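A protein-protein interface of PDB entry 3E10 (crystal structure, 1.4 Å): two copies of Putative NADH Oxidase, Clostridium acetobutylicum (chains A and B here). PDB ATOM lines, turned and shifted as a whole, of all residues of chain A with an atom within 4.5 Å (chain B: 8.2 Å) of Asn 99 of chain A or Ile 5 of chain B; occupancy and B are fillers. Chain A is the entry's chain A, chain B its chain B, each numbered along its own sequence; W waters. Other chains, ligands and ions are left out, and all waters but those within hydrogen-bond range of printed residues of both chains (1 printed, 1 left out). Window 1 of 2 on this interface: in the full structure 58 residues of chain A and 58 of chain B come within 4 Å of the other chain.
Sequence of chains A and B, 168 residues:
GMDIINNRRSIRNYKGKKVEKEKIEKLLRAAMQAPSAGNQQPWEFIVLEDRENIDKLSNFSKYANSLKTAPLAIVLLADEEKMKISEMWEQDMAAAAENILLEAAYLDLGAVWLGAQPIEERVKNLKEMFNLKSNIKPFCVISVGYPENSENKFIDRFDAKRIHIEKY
Among the printed residues, merely in contact across the chains: Glu 98 of chain A with Pro 35 of chain B, Leu 102 of chain A with Leu 102 of chain B, Gln 33 of chain A with Asn 6 of chain B, Gln 33 of chain A with Ile 5 of chain B, Leu 102 of chain A with Asn 99 of chain B, Asn 99 of chain A with Leu 102 of chain B, Ala 34 of chain A with Arg 8 of chain B, Asn 99 of chain A with Ile 5 of chain B, Glu 103 of chain A with Ile 5 of chain B, Ala 30 of chain A with Ile 5 of chain B, Gln 33 of chain A with Phe 154 of chain B, Glu 98 of chain A with Ala 95 of chain B, Ala 95 of chain A with Glu 98 of chain B and Gln 33 of chain A with Arg 9 of chain B.
Water W1 lies within hydrogen-bond range of the backbone carbonyl oxygen of Gln 33 of chain A (2.8 Å), the backbone carbonyl oxygen of Ile 5 of chain B (2.8 Å), the guanidinium group of Arg 8 of chain B (3.0 Å) and the side-chain amide nitrogen of Asn 99 of chain A (3.0 Å).
Ala 96 of chain A touches none of the printed residues of chain B. Asn 99 of chain A touches just these residues of chain B: Ile 5, Glu 98 and Leu 102. Ile 100 of chain A touches none of the printed residues of chain B. Of the printed residues of chain A, Ile 5 of chain B touches Ala 30, Gln 33, Asn 99 and Glu 103. Printed residues of chain A within 4 Å of Pro 35 of chain B: Glu 98. Printed residues of chain A within 4 Å of Leu 102 of chain B: Asn 99 and Leu 102. Printed residues of chain A within 4 Å of Phe 154 of chain B: Gln 33. The nearest printed residue of chain A that does not touch Leu 102 of chain B is Glu 98 of chain A (5.5 Å).
Printed residues of chain A that touch a printed residue of chain B: Ala 30, Gln 33, Ala 34, Ala 95, Glu 98, Asn 99, Leu 102 and Glu 103. Along chain A the printed residues that touch a printed residue of chain B span positions 30 to 103. Hydrophobic or aromatic side chains of chain B within 4 Å of the printed part of chain A: Ile 5, Pro 35, Leu 102 and Phe 154. Among the printed residues, 18 pairs touch across the chains. Among the printed residues, no Asp or Glu carboxylate lies within 4 Å of a Lys or Arg side-chain nitrogen of the other chain.
The backbone carbonyl oxygen (O) of Gln 33 of chain A sits at hydrogen-bond distance from the guanidinium group (NH2) of Arg 8 of chain B (2.9 Å). O of Ile 155 of chain B sits at hydrogen-bond distance from NE2 of Gln 33 of chain A, 2.8 Å away. The side-chain amide oxygen of Asn 99 of chain A sits close to the side-chain carboxylate of Glu 98 of chain B, 2.6 Å away. OD1 of Asn 99 of chain B lies close to OE2 of Glu 98 of chain A.
Ala 95 of chain A touches Glu 98 of chain B, and with the chains exchanged Glu 98 of chain A touches Ala 95 of chain B. Glu 98 of chain A touches Asn 99 of chain B, and with the chains exchanged Asn 99 of chain A touches Glu 98 of chain B. Asn 99 of chain A touches Leu 102 of chain B, and with the chains exchanged Leu 102 of chain A touches Asn 99 of chain B. Leu 102 of chain A touches its own counterpart, Leu 102 of chain B. Positions printed for both chains: 95, 98, 99, 101 and 102. Of the 18 pairs that touch across the chains among the printed residues, 7 have their exchanged pair printed and touching as well.
The backbone NH (N) of Phe 154 of chain B sits at hydrogen-bond distance from the side-chain amide oxygen (OD1) of Asn 7 of chain B (2.9 Å). The guanidinium group of Arg 9 of chain B sits at hydrogen-bond distance from the backbone carbonyl oxygen of Lys 153 of chain B. O of Asn 6 of chain B lies within hydrogen-bond range of NH1 of Arg 9 of chain B (3.1 Å). The backbone NH (N) of Ala 34 of chain A lies close to the side-chain amide nitrogen (ND2) of Asn 99 of chain A (3.5 Å). The side-chain amide nitrogen (ND2) of Asn 99 of chain A lies within hydrogen-bond range of the backbone carbonyl oxygen (O) of Ala 30 of chain A. The guanidinium group of Arg 8 of chain B is in salt-bridge range of the side-chain carboxylate of Glu 98 of chain B (3.9 Å).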
ATOM      1  N   ALA A  30      -4.449   1.059 -19.132  1.00  0.00           N
ATOM      2  CA  ALA A  30      -3.449   2.124 -19.032  1.00  0.00           C
ATOM      3  C   ALA A  30      -2.035   1.521 -18.962  1.00  0.00           C
ATOM      4  O   ALA A  30      -1.115   1.972 -19.649  1.00  0.00           O
ATOM      5  CB  ALA A  30      -3.717   3.017 -17.775  1.00  0.00           C
ATOM      6  N   ALA A  31      -1.873   0.468 -18.168  1.00  0.00           N
ATOM      7  CA  ALA A  31      -0.594  -0.206 -18.012  1.00  0.00           C
ATOM      8  C   ALA A  31      -0.090  -0.664 -19.369  1.00  0.00           C
ATOM      9  O   ALA A  31       1.073  -0.467 -19.707  1.00  0.00           O
ATOM     10  CB  ALA A  31      -0.737  -1.406 -17.084  1.00  0.00           C
ATOM     11  N   GLN A  33      -0.671   0.333 -22.299  1.00  0.00           N
ATOM     12  CA  GLN A  33      -0.309   1.381 -23.244  1.00  0.00           C
ATOM     13  C   GLN A  33       1.069   1.970 -22.992  1.00  0.00           C
ATOM     14  O   GLN A  33       1.485   2.884 -23.715  1.00  0.00           O
ATOM     15  CB  GLN A  33      -1.311   2.527 -23.223  1.00  0.00           C
ATOM     16  CG  GLN A  33      -2.698   2.150 -23.736  1.00  0.00           C
ATOM     17  CD  GLN A  33      -2.659   1.629 -25.139  1.00  0.00           C
ATOM     18  OE1 GLN A  33      -3.089   0.489 -25.396  1.00  0.00           O
ATOM     19  NE2 GLN A  33      -2.158   2.450 -26.082  1.00  0.00           N
ATOM     20  N   ALA A  34       1.774   1.506 -21.965  1.00  0.00           N
ATOM     21  CA  ALA A  34       3.144   2.002 -21.711  1.00  0.00           C
ATOM     22  C   ALA A  34       4.100   1.720 -22.858  1.00  0.00           C
ATOM     23  O   ALA A  34       3.920   0.756 -23.609  1.00  0.00           O
ATOM     24  CB  ALA A  34       3.701   1.368 -20.442  1.00  0.00           C
ATOM     25  N   ALA A  95       7.360   2.032 -16.351  1.00  0.00           N
ATOM     26  CA  ALA A  95       6.486   2.869 -17.157  1.00  0.00           C
ATOM     27  C   ALA A  95       5.016   2.424 -17.038  1.00  0.00           C
ATOM     28  O   ALA A  95       4.108   3.246 -16.969  1.00  0.00           O
ATOM     29  CB  ALA A  95       6.957   2.857 -18.624  1.00  0.00           C
ATOM     30  N   ALA A  96       4.793   1.120 -17.069  1.00  0.00           N
ATOM     31  CA  ALA A  96       3.471   0.545 -16.917  1.00  0.00           C
ATOM     32  C   ALA A  96       2.919   0.888 -15.544  1.00  0.00           C
ATOM     33  O   ALA A  96       1.752   1.258 -15.412  1.00  0.00           O
ATOM     34  CB  ALA A  96       3.512  -1.005 -17.142  1.00  0.00           C
ATOM     35  N   ALA A  97       3.764   0.748 -14.513  1.00  0.00           N
ATOM     36  CA  ALA A  97       3.374   1.092 -13.150  1.00  0.00           C
ATOM     37  C   ALA A  97       2.947   2.557 -13.039  1.00  0.00           C
ATOM     38  O   ALA A  97       1.886   2.888 -12.455  1.00  0.00           O
ATOM     39  CB  ALA A  97       4.501   0.768 -12.175  1.00  0.00           C
ATOM     40  N   GLU A  98       3.741   3.441 -13.618  1.00  0.00           N
ATOM     41  CA  GLU A  98       3.413   4.866 -13.577  1.00  0.00           C
ATOM     42  C   GLU A  98       2.100   5.144 -14.291  1.00  0.00           C
ATOM     43  O   GLU A  98       1.299   5.969 -13.813  1.00  0.00           O
ATOM     44  CB  GLU A  98       4.577   5.729 -14.095  1.00  0.00           C
ATOM     45  CG  GLU A  98       4.323   7.237 -14.084  1.00  0.00           C
ATOM     46  CD  GLU A  98       4.150   7.848 -12.708  1.00  0.00           C
ATOM     47  OE1 GLU A  98       4.186   7.105 -11.700  1.00  0.00           O
ATOM     48  OE2 GLU A  98       3.944   9.115 -12.624  1.00  0.00           O
ATOM     49  N   ASN A  99       1.840   4.464 -15.406  1.00  0.00           N
ATOM     50  CA  ASN A  99       0.554   4.644 -16.081  1.00  0.00           C
ATOM     51  C   ASN A  99      -0.609   4.202 -15.194  1.00  0.00           C
ATOM     52  O   ASN A  99      -1.655   4.831 -15.200  1.00  0.00           O
ATOM     53  CB  ASN A  99       0.510   3.878 -17.417  1.00  0.00           C
ATOM     54  CG  ASN A  99       1.160   4.624 -18.567  1.00  0.00           C
ATOM     55  OD1 ASN A  99       1.827   5.640 -18.375  1.00  0.00           O
ATOM     56  ND2 ASN A  99       0.954   4.112 -19.793  1.00  0.00           N
ATOM     57  N   ILE A 100      -0.455   3.089 -14.486  1.00  0.00           N
ATOM     58  CA  ILE A 100      -1.505   2.636 -13.554  1.00  0.00           C
ATOM     59  C   ILE A 100      -1.750   3.707 -12.500  1.00  0.00           C
ATOM     60  O   ILE A 100      -2.895   4.022 -12.196  1.00  0.00           O
ATOM     61  CB  ILE A 100      -1.147   1.299 -12.888  1.00  0.00           C
ATOM     62  CG1 ILE A 100      -1.102   0.183 -13.949  1.00  0.00           C
ATOM     63  CG2 ILE A 100      -2.150   0.974 -11.754  1.00  0.00           C
ATOM     64  CD1 ILE A 100      -0.575  -1.156 -13.419  1.00  0.00           C
ATOM     65  N   LEU A 101      -0.681   4.230 -11.910  1.00  0.00           N
ATOM     66  CA  LEU A 101      -0.829   5.242 -10.861  1.00  0.00           C
ATOM     67  C   LEU A 101      -1.555   6.484 -11.345  1.00  0.00           C
ATOM     68  O   LEU A 101      -2.390   7.063 -10.630  1.00  0.00           O
ATOM     69  CB  LEU A 101       0.543   5.641 -10.295  1.00  0.00           C
ATOM     70  CG  LEU A 101       1.325   4.523  -9.591  1.00  0.00           C
ATOM     71  CD1 LEU A 101       2.643   5.078  -9.070  1.00  0.00           C
ATOM     72  CD2 LEU A 101       0.550   3.833  -8.480  1.00  0.00           C
ATOM     73  N   LEU A 102      -1.198   6.930 -12.544  1.00  0.00           N
ATOM     74  CA  LEU A 102      -1.798   8.110 -13.086  1.00  0.00           C
ATOM     75  C   LEU A 102      -3.273   7.855 -13.404  1.00  0.00           C
ATOM     76  O   LEU A 102      -4.144   8.710 -13.164  1.00  0.00           O
ATOM     77  CB  LEU A 102      -1.017   8.619 -14.286  1.00  0.00           C
ATOM     78  CG  LEU A 102       0.389   9.167 -14.007  1.00  0.00           C
ATOM     79  CD1 LEU A 102       1.116   9.379 -15.330  1.00  0.00           C
ATOM     80  CD2 LEU A 102       0.329  10.453 -13.210  1.00  0.00           C
ATOM     81  N   GLU A 103      -3.566   6.714 -14.031  1.00  0.00           N
ATOM     82  CA  GLU A 103      -4.953   6.371 -14.362  1.00  0.00           C
ATOM     83  C   GLU A 103      -5.775   6.248 -13.060  1.00  0.00           C
ATOM     84  O   GLU A 103      -6.930   6.671 -13.017  1.00  0.00           O
ATOM     85  CB  GLU A 103      -5.029   5.090 -15.228  1.00  0.00           C
ATOM     86  CG  GLU A 103      -6.444   4.680 -15.613  1.00  0.00           C
ATOM     87  CD  GLU A 103      -7.055   5.564 -16.636  1.00  0.00           C
ATOM     88  OE1 GLU A 103      -6.321   6.347 -17.261  1.00  0.00           O
ATOM     89  OE2 GLU A 103      -8.283   5.455 -16.826  1.00  0.00           O
ATOM     90  N   MET B   2      -9.599  13.780 -21.839  1.00  0.00           N
ATOM     91  CA  MET B   2      -8.163  13.505 -21.534  1.00  0.00           C
ATOM     92  C   MET B   2      -7.882  12.083 -21.944  1.00  0.00           C
ATOM     93  O   MET B   2      -8.428  11.138 -21.351  1.00  0.00           O
ATOM     94  CB  MET B   2      -7.854  13.714 -20.042  1.00  0.00           C
ATOM     95  N   ASP B   3      -7.039  11.932 -22.971  1.00  0.00           N
ATOM     96  CA  ASP B   3      -6.808  10.627 -23.578  1.00  0.00           C
ATOM     97  C   ASP B   3      -5.321  10.407 -23.807  1.00  0.00           C
ATOM     98  O   ASP B   3      -4.903   9.645 -24.684  1.00  0.00           O
ATOM     99  CB  ASP B   3      -7.558  10.558 -24.880  1.00  0.00           C
ATOM    100  N   ILE B   4      -4.520  11.062 -22.989  1.00  0.00           N
ATOM    101  CA  ILE B   4      -3.095  11.101 -23.195  1.00  0.00           C
ATOM    102  C   ILE B   4      -2.428   9.750 -22.978  1.00  0.00           C
ATOM    103  O   ILE B   4      -1.508   9.411 -23.708  1.00  0.00           O
ATOM    104  CB  ILE B   4      -2.478  12.200 -22.309  1.00  0.00           C
ATOM    105  CG1 ILE B   4      -3.066  13.571 -22.668  1.00  0.00           C
ATOM    106  CG2 ILE B   4      -1.043  12.225 -22.421  1.00  0.00           C
ATOM    107  CD1 ILE B   4      -2.934  13.970 -24.135  1.00  0.00           C
ATOM    108  N   ILE B   5      -2.855   8.960 -21.985  1.00  0.00           N
ATOM    109  CA  ILE B   5      -2.258   7.639 -21.811  1.00  0.00           C
ATOM    110  C   ILE B   5      -2.485   6.780 -23.057  1.00  0.00           C
ATOM    111  O   ILE B   5      -1.574   6.094 -23.494  1.00  0.00           O
ATOM    112  CB  ILE B   5      -2.753   6.941 -20.523  1.00  0.00           C
ATOM    113  CG1 ILE B   5      -2.224   7.694 -19.294  1.00  0.00           C
ATOM    114  CG2 ILE B   5      -2.412   5.437 -20.513  1.00  0.00           C
ATOM    115  CD1 ILE B   5      -2.753   7.214 -17.889  1.00  0.00           C
ATOM    116  N   ASN B   6      -3.685   6.823 -23.649  1.00  0.00           N
ATOM    117  CA  ASN B   6      -3.957   6.051 -24.853  1.00  0.00           C
ATOM    118  C   ASN B   6      -3.233   6.565 -26.094  1.00  0.00           C
ATOM    119  O   ASN B   6      -2.898   5.774 -26.998  1.00  0.00           O
ATOM    120  CB  ASN B   6      -5.454   6.063 -25.172  1.00  0.00           C
ATOM    121  CG  ASN B   6      -6.236   5.080 -24.331  1.00  0.00           C
ATOM    122  OD1 ASN B   6      -5.697   4.147 -23.772  1.00  0.00           O
ATOM    123  ND2 ASN B   6      -7.540   5.295 -24.261  1.00  0.00           N
ATOM    124  N   ASN B   7      -3.061   7.884 -26.185  1.00  0.00           N
ATOM    125  CA  ASN B   7      -2.586   8.491 -27.426  1.00  0.00           C
ATOM    126  C   ASN B   7      -1.083   8.734 -27.490  1.00  0.00           C
ATOM    127  O   ASN B   7      -0.554   8.976 -28.557  1.00  0.00           O
ATOM    128  CB  ASN B   7      -3.353   9.786 -27.705  1.00  0.00           C
ATOM    129  CG  ASN B   7      -4.765   9.530 -28.202  1.00  0.00           C
ATOM    130  OD1 ASN B   7      -4.964   8.907 -29.229  1.00  0.00           O
ATOM    131  ND2 ASN B   7      -5.751  10.028 -27.472  1.00  0.00           N
ATOM    132  N   ARG B   8      -0.397   8.686 -26.347  1.00  0.00           N
ATOM    133  CA  ARG B   8       1.050   8.885 -26.351  1.00  0.00           C
ATOM    134  C   ARG B   8       1.724   7.846 -27.258  1.00  0.00           C
ATOM    135  O   ARG B   8       1.556   6.636 -27.044  1.00  0.00           O
ATOM    136  CB  ARG B   8       1.573   8.706 -24.950  1.00  0.00           C
ATOM    137  CG  ARG B   8       3.116   8.800 -24.813  1.00  0.00           C
ATOM    138  CD  ARG B   8       3.711   7.801 -23.816  1.00  0.00           C
ATOM    139  NE  ARG B   8       3.340   6.412 -24.135  1.00  0.00           N
ATOM    140  CZ  ARG B   8       3.890   5.657 -25.083  1.00  0.00           C
ATOM    141  NH1 ARG B   8       4.822   6.145 -25.883  1.00  0.00           N
ATOM    142  NH2 ARG B   8       3.458   4.415 -25.260  1.00  0.00           N
ATOM    143  N   ARG B   9       2.516   8.332 -28.220  1.00  0.00           N
ATOM    144  CA  ARG B   9       3.253   7.445 -29.117  1.00  0.00           C
ATOM    145  C   ARG B   9       4.726   7.835 -29.138  1.00  0.00           C
ATOM    146  O   ARG B   9       5.090   8.986 -28.886  1.00  0.00           O
ATOM    147  CB  ARG B   9       2.707   7.521 -30.566  1.00  0.00           C
ATOM    148  CG  ARG B   9       1.269   7.033 -30.743  1.00  0.00           C
ATOM    149  CD  ARG B   9       1.135   5.556 -30.969  1.00  0.00           C
ATOM    150  NE  ARG B   9       1.507   4.714 -29.833  1.00  0.00           N
ATOM    151  CZ  ARG B   9       0.680   4.420 -28.832  1.00  0.00           C
ATOM    152  NH1 ARG B   9      -0.560   4.911 -28.775  1.00  0.00           N
ATOM    153  NH2 ARG B   9       1.110   3.646 -27.857  1.00  0.00           N
ATOM    154  N   PRO B  35       6.824   9.480  -8.812  1.00  0.00           N
ATOM    155  CA  PRO B  35       7.105   8.789  -7.581  1.00  0.00           C
ATOM    156  C   PRO B  35       8.571   8.346  -7.585  1.00  0.00           C
ATOM    157  O   PRO B  35       9.203   8.241  -8.640  1.00  0.00           O
ATOM    158  CB  PRO B  35       6.166   7.591  -7.616  1.00  0.00           C
ATOM    159  CG  PRO B  35       6.047   7.294  -9.069  1.00  0.00           C
ATOM    160  CD  PRO B  35       5.984   8.675  -9.724  1.00  0.00           C
ATOM    161  N   ALA B  94      12.593   5.798 -14.738  1.00  0.00           N
ATOM    162  CA  ALA B  94      11.626   5.360 -15.721  1.00  0.00           C
ATOM    163  C   ALA B  94      10.260   6.032 -15.495  1.00  0.00           C
ATOM    164  O   ALA B  94       9.583   6.420 -16.448  1.00  0.00           O
ATOM    165  CB  ALA B  94      11.519   3.796 -15.673  1.00  0.00           C
ATOM    166  N   ALA B  95       9.882   6.183 -14.225  1.00  0.00           N
ATOM    167  CA  ALA B  95       8.614   6.855 -13.915  1.00  0.00           C
ATOM    168  C   ALA B  95       8.675   8.324 -14.342  1.00  0.00           C
ATOM    169  O   ALA B  95       7.707   8.862 -14.875  1.00  0.00           O
ATOM    170  CB  ALA B  95       8.309   6.707 -12.405  1.00  0.00           C
ATOM    171  N   GLU B  98       8.402   8.490 -18.164  1.00  0.00           N
ATOM    172  CA  GLU B  98       7.035   8.281 -18.607  1.00  0.00           C
ATOM    173  C   GLU B  98       6.233   9.552 -18.368  1.00  0.00           C
ATOM    174  O   GLU B  98       5.415   9.916 -19.207  1.00  0.00           O
ATOM    175  CB  GLU B  98       6.404   7.056 -17.919  1.00  0.00           C
ATOM    176  CG  GLU B  98       4.942   6.749 -18.350  1.00  0.00           C
ATOM    177  CD  GLU B  98       4.764   6.413 -19.834  1.00  0.00           C
ATOM    178  OE1 GLU B  98       5.745   6.429 -20.601  1.00  0.00           O
ATOM    179  OE2 GLU B  98       3.594   6.156 -20.247  1.00  0.00           O
ATOM    180  N   ASN B  99       6.461  10.225 -17.235  1.00  0.00           N
ATOM    181  CA  ASN B  99       5.770  11.495 -17.035  1.00  0.00           C
ATOM    182  C   ASN B  99       6.105  12.518 -18.132  1.00  0.00           C
ATOM    183  O   ASN B  99       5.244  13.283 -18.586  1.00  0.00           O
ATOM    184  CB  ASN B  99       6.069  12.098 -15.675  1.00  0.00           C
ATOM    185  CG  ASN B  99       5.230  11.504 -14.560  1.00  0.00           C
ATOM    186  OD1 ASN B  99       4.511  10.501 -14.734  1.00  0.00           O
ATOM    187  ND2 ASN B  99       5.321  12.136 -13.383  1.00  0.00           N
ATOM    188  N   LEU B 101       7.017  11.864 -21.225  1.00  0.00           N
ATOM    189  CA  LEU B 101       6.386  11.471 -22.467  1.00  0.00           C
ATOM    190  C   LEU B 101       4.907  11.829 -22.445  1.00  0.00           C
ATOM    191  O   LEU B 101       4.359  12.251 -23.468  1.00  0.00           O
ATOM    192  CB  LEU B 101       6.555   9.977 -22.692  1.00  0.00           C
ATOM    193  CG  LEU B 101       7.977   9.445 -22.846  1.00  0.00           C
ATOM    194  CD1 LEU B 101       7.909   7.932 -23.017  1.00  0.00           C
ATOM    195  CD2 LEU B 101       8.767  10.130 -24.009  1.00  0.00           C
ATOM    196  N   LEU B 102       4.230  11.571 -21.331  1.00  0.00           N
ATOM    197  CA  LEU B 102       2.811  11.897 -21.255  1.00  0.00           C
ATOM    198  C   LEU B 102       2.550  13.397 -21.318  1.00  0.00           C
ATOM    199  O   LEU B 102       1.629  13.843 -22.003  1.00  0.00           O
ATOM    200  CB  LEU B 102       2.200  11.277 -20.006  1.00  0.00           C
ATOM    201  CG  LEU B 102       2.159   9.746 -19.980  1.00  0.00           C
ATOM    202  CD1 LEU B 102       1.804   9.272 -18.578  1.00  0.00           C
ATOM    203  CD2 LEU B 102       1.190   9.166 -21.040  1.00  0.00           C
ATOM    204  N   ALA B 105       2.841  14.607 -24.907  1.00  0.00           N
ATOM    205  CA  ALA B 105       1.619  14.351 -25.675  1.00  0.00           C
ATOM    206  C   ALA B 105       0.530  15.365 -25.289  1.00  0.00           C
ATOM    207  O   ALA B 105      -0.180  15.901 -26.174  1.00  0.00           O
ATOM    208  CB  ALA B 105       1.165  12.917 -25.504  1.00  0.00           C
ATOM    209  N   TYR B 106       0.404  15.650 -23.987  1.00  0.00           N
ATOM    210  CA  TYR B 106      -0.561  16.647 -23.498  1.00  0.00           C
ATOM    211  C   TYR B 106      -0.359  18.023 -24.150  1.00  0.00           C
ATOM    212  O   TYR B 106      -1.335  18.721 -24.460  1.00  0.00           O
ATOM    213  CB  TYR B 106      -0.492  16.701 -21.979  1.00  0.00           C
ATOM    214  CG  TYR B 106      -1.306  17.810 -21.374  1.00  0.00           C
ATOM    215  CD1 TYR B 106      -2.677  17.726 -21.322  1.00  0.00           C
ATOM    216  CD2 TYR B 106      -0.692  18.947 -20.877  1.00  0.00           C
ATOM    217  CE1 TYR B 106      -3.435  18.787 -20.774  1.00  0.00           C
ATOM    218  CE2 TYR B 106      -1.410  19.964 -20.323  1.00  0.00           C
ATOM    219  CZ  TYR B 106      -2.763  19.884 -20.272  1.00  0.00           C
ATOM    220  OH  TYR B 106      -3.456  20.961 -19.729  1.00  0.00           O
ATOM    221  N   LYS B 153      -1.627   9.113 -31.448  1.00  0.00           N
ATOM    222  CA  LYS B 153      -2.898   8.470 -31.764  1.00  0.00           C
ATOM    223  C   LYS B 153      -2.970   7.157 -31.005  1.00  0.00           C
ATOM    224  O   LYS B 153      -1.952   6.634 -30.567  1.00  0.00           O
ATOM    225  CB  LYS B 153      -3.007   8.178 -33.261  1.00  0.00           C
ATOM    226  CG  LYS B 153      -2.131   7.032 -33.771  1.00  0.00           C
ATOM    227  CD  LYS B 153      -2.296   6.836 -35.291  1.00  0.00           C
ATOM    228  CE  LYS B 153      -1.366   5.777 -35.822  1.00  0.00           C
ATOM    229  NZ  LYS B 153      -1.314   5.768 -37.323  1.00  0.00           N
ATOM    230  N   PHE B 154      -4.164   6.613 -30.880  1.00  0.00           N
ATOM    231  CA  PHE B 154      -4.401   5.410 -30.090  1.00  0.00           C
ATOM    232  C   PHE B 154      -4.080   4.171 -30.913  1.00  0.00           C
ATOM    233  O   PHE B 154      -4.771   3.872 -31.892  1.00  0.00           O
ATOM    234  CB  PHE B 154      -5.861   5.402 -29.614  1.00  0.00           C
ATOM    235  CG  PHE B 154      -6.265   4.209 -28.785  1.00  0.00           C
ATOM    236  CD1 PHE B 154      -5.452   3.686 -27.808  1.00  0.00           C
ATOM    237  CD2 PHE B 154      -7.516   3.657 -28.936  1.00  0.00           C
ATOM    238  CE1 PHE B 154      -5.838   2.626 -27.015  1.00  0.00           C
ATOM    239  CE2 PHE B 154      -7.914   2.589 -28.153  1.00  0.00           C
ATOM    240  CZ  PHE B 154      -7.073   2.082 -27.181  1.00  0.00           C
ATOM    241  N   ILE B 155      -3.010   3.468 -30.523  1.00  0.00           N
ATOM    242  CA  ILE B 155      -2.732   2.102 -30.975  1.00  0.00           C
ATOM    243  C   ILE B 155      -3.092   1.237 -29.755  1.00  0.00           C
ATOM    244  O   ILE B 155      -2.498   1.367 -28.693  1.00  0.00           O
ATOM    245  CB  ILE B 155      -1.273   1.874 -31.403  1.00  0.00           C
ATOM    246  CG1 ILE B 155      -0.925   2.748 -32.617  1.00  0.00           C
ATOM    247  CG2 ILE B 155      -1.014   0.421 -31.651  1.00  0.00           C
ATOM    248  CD1 ILE B 155       0.541   2.670 -33.042  1.00  0.00           C
HETATM  249  O   HOH W   1       1.001   5.377 -22.562  1.00  0.00           O
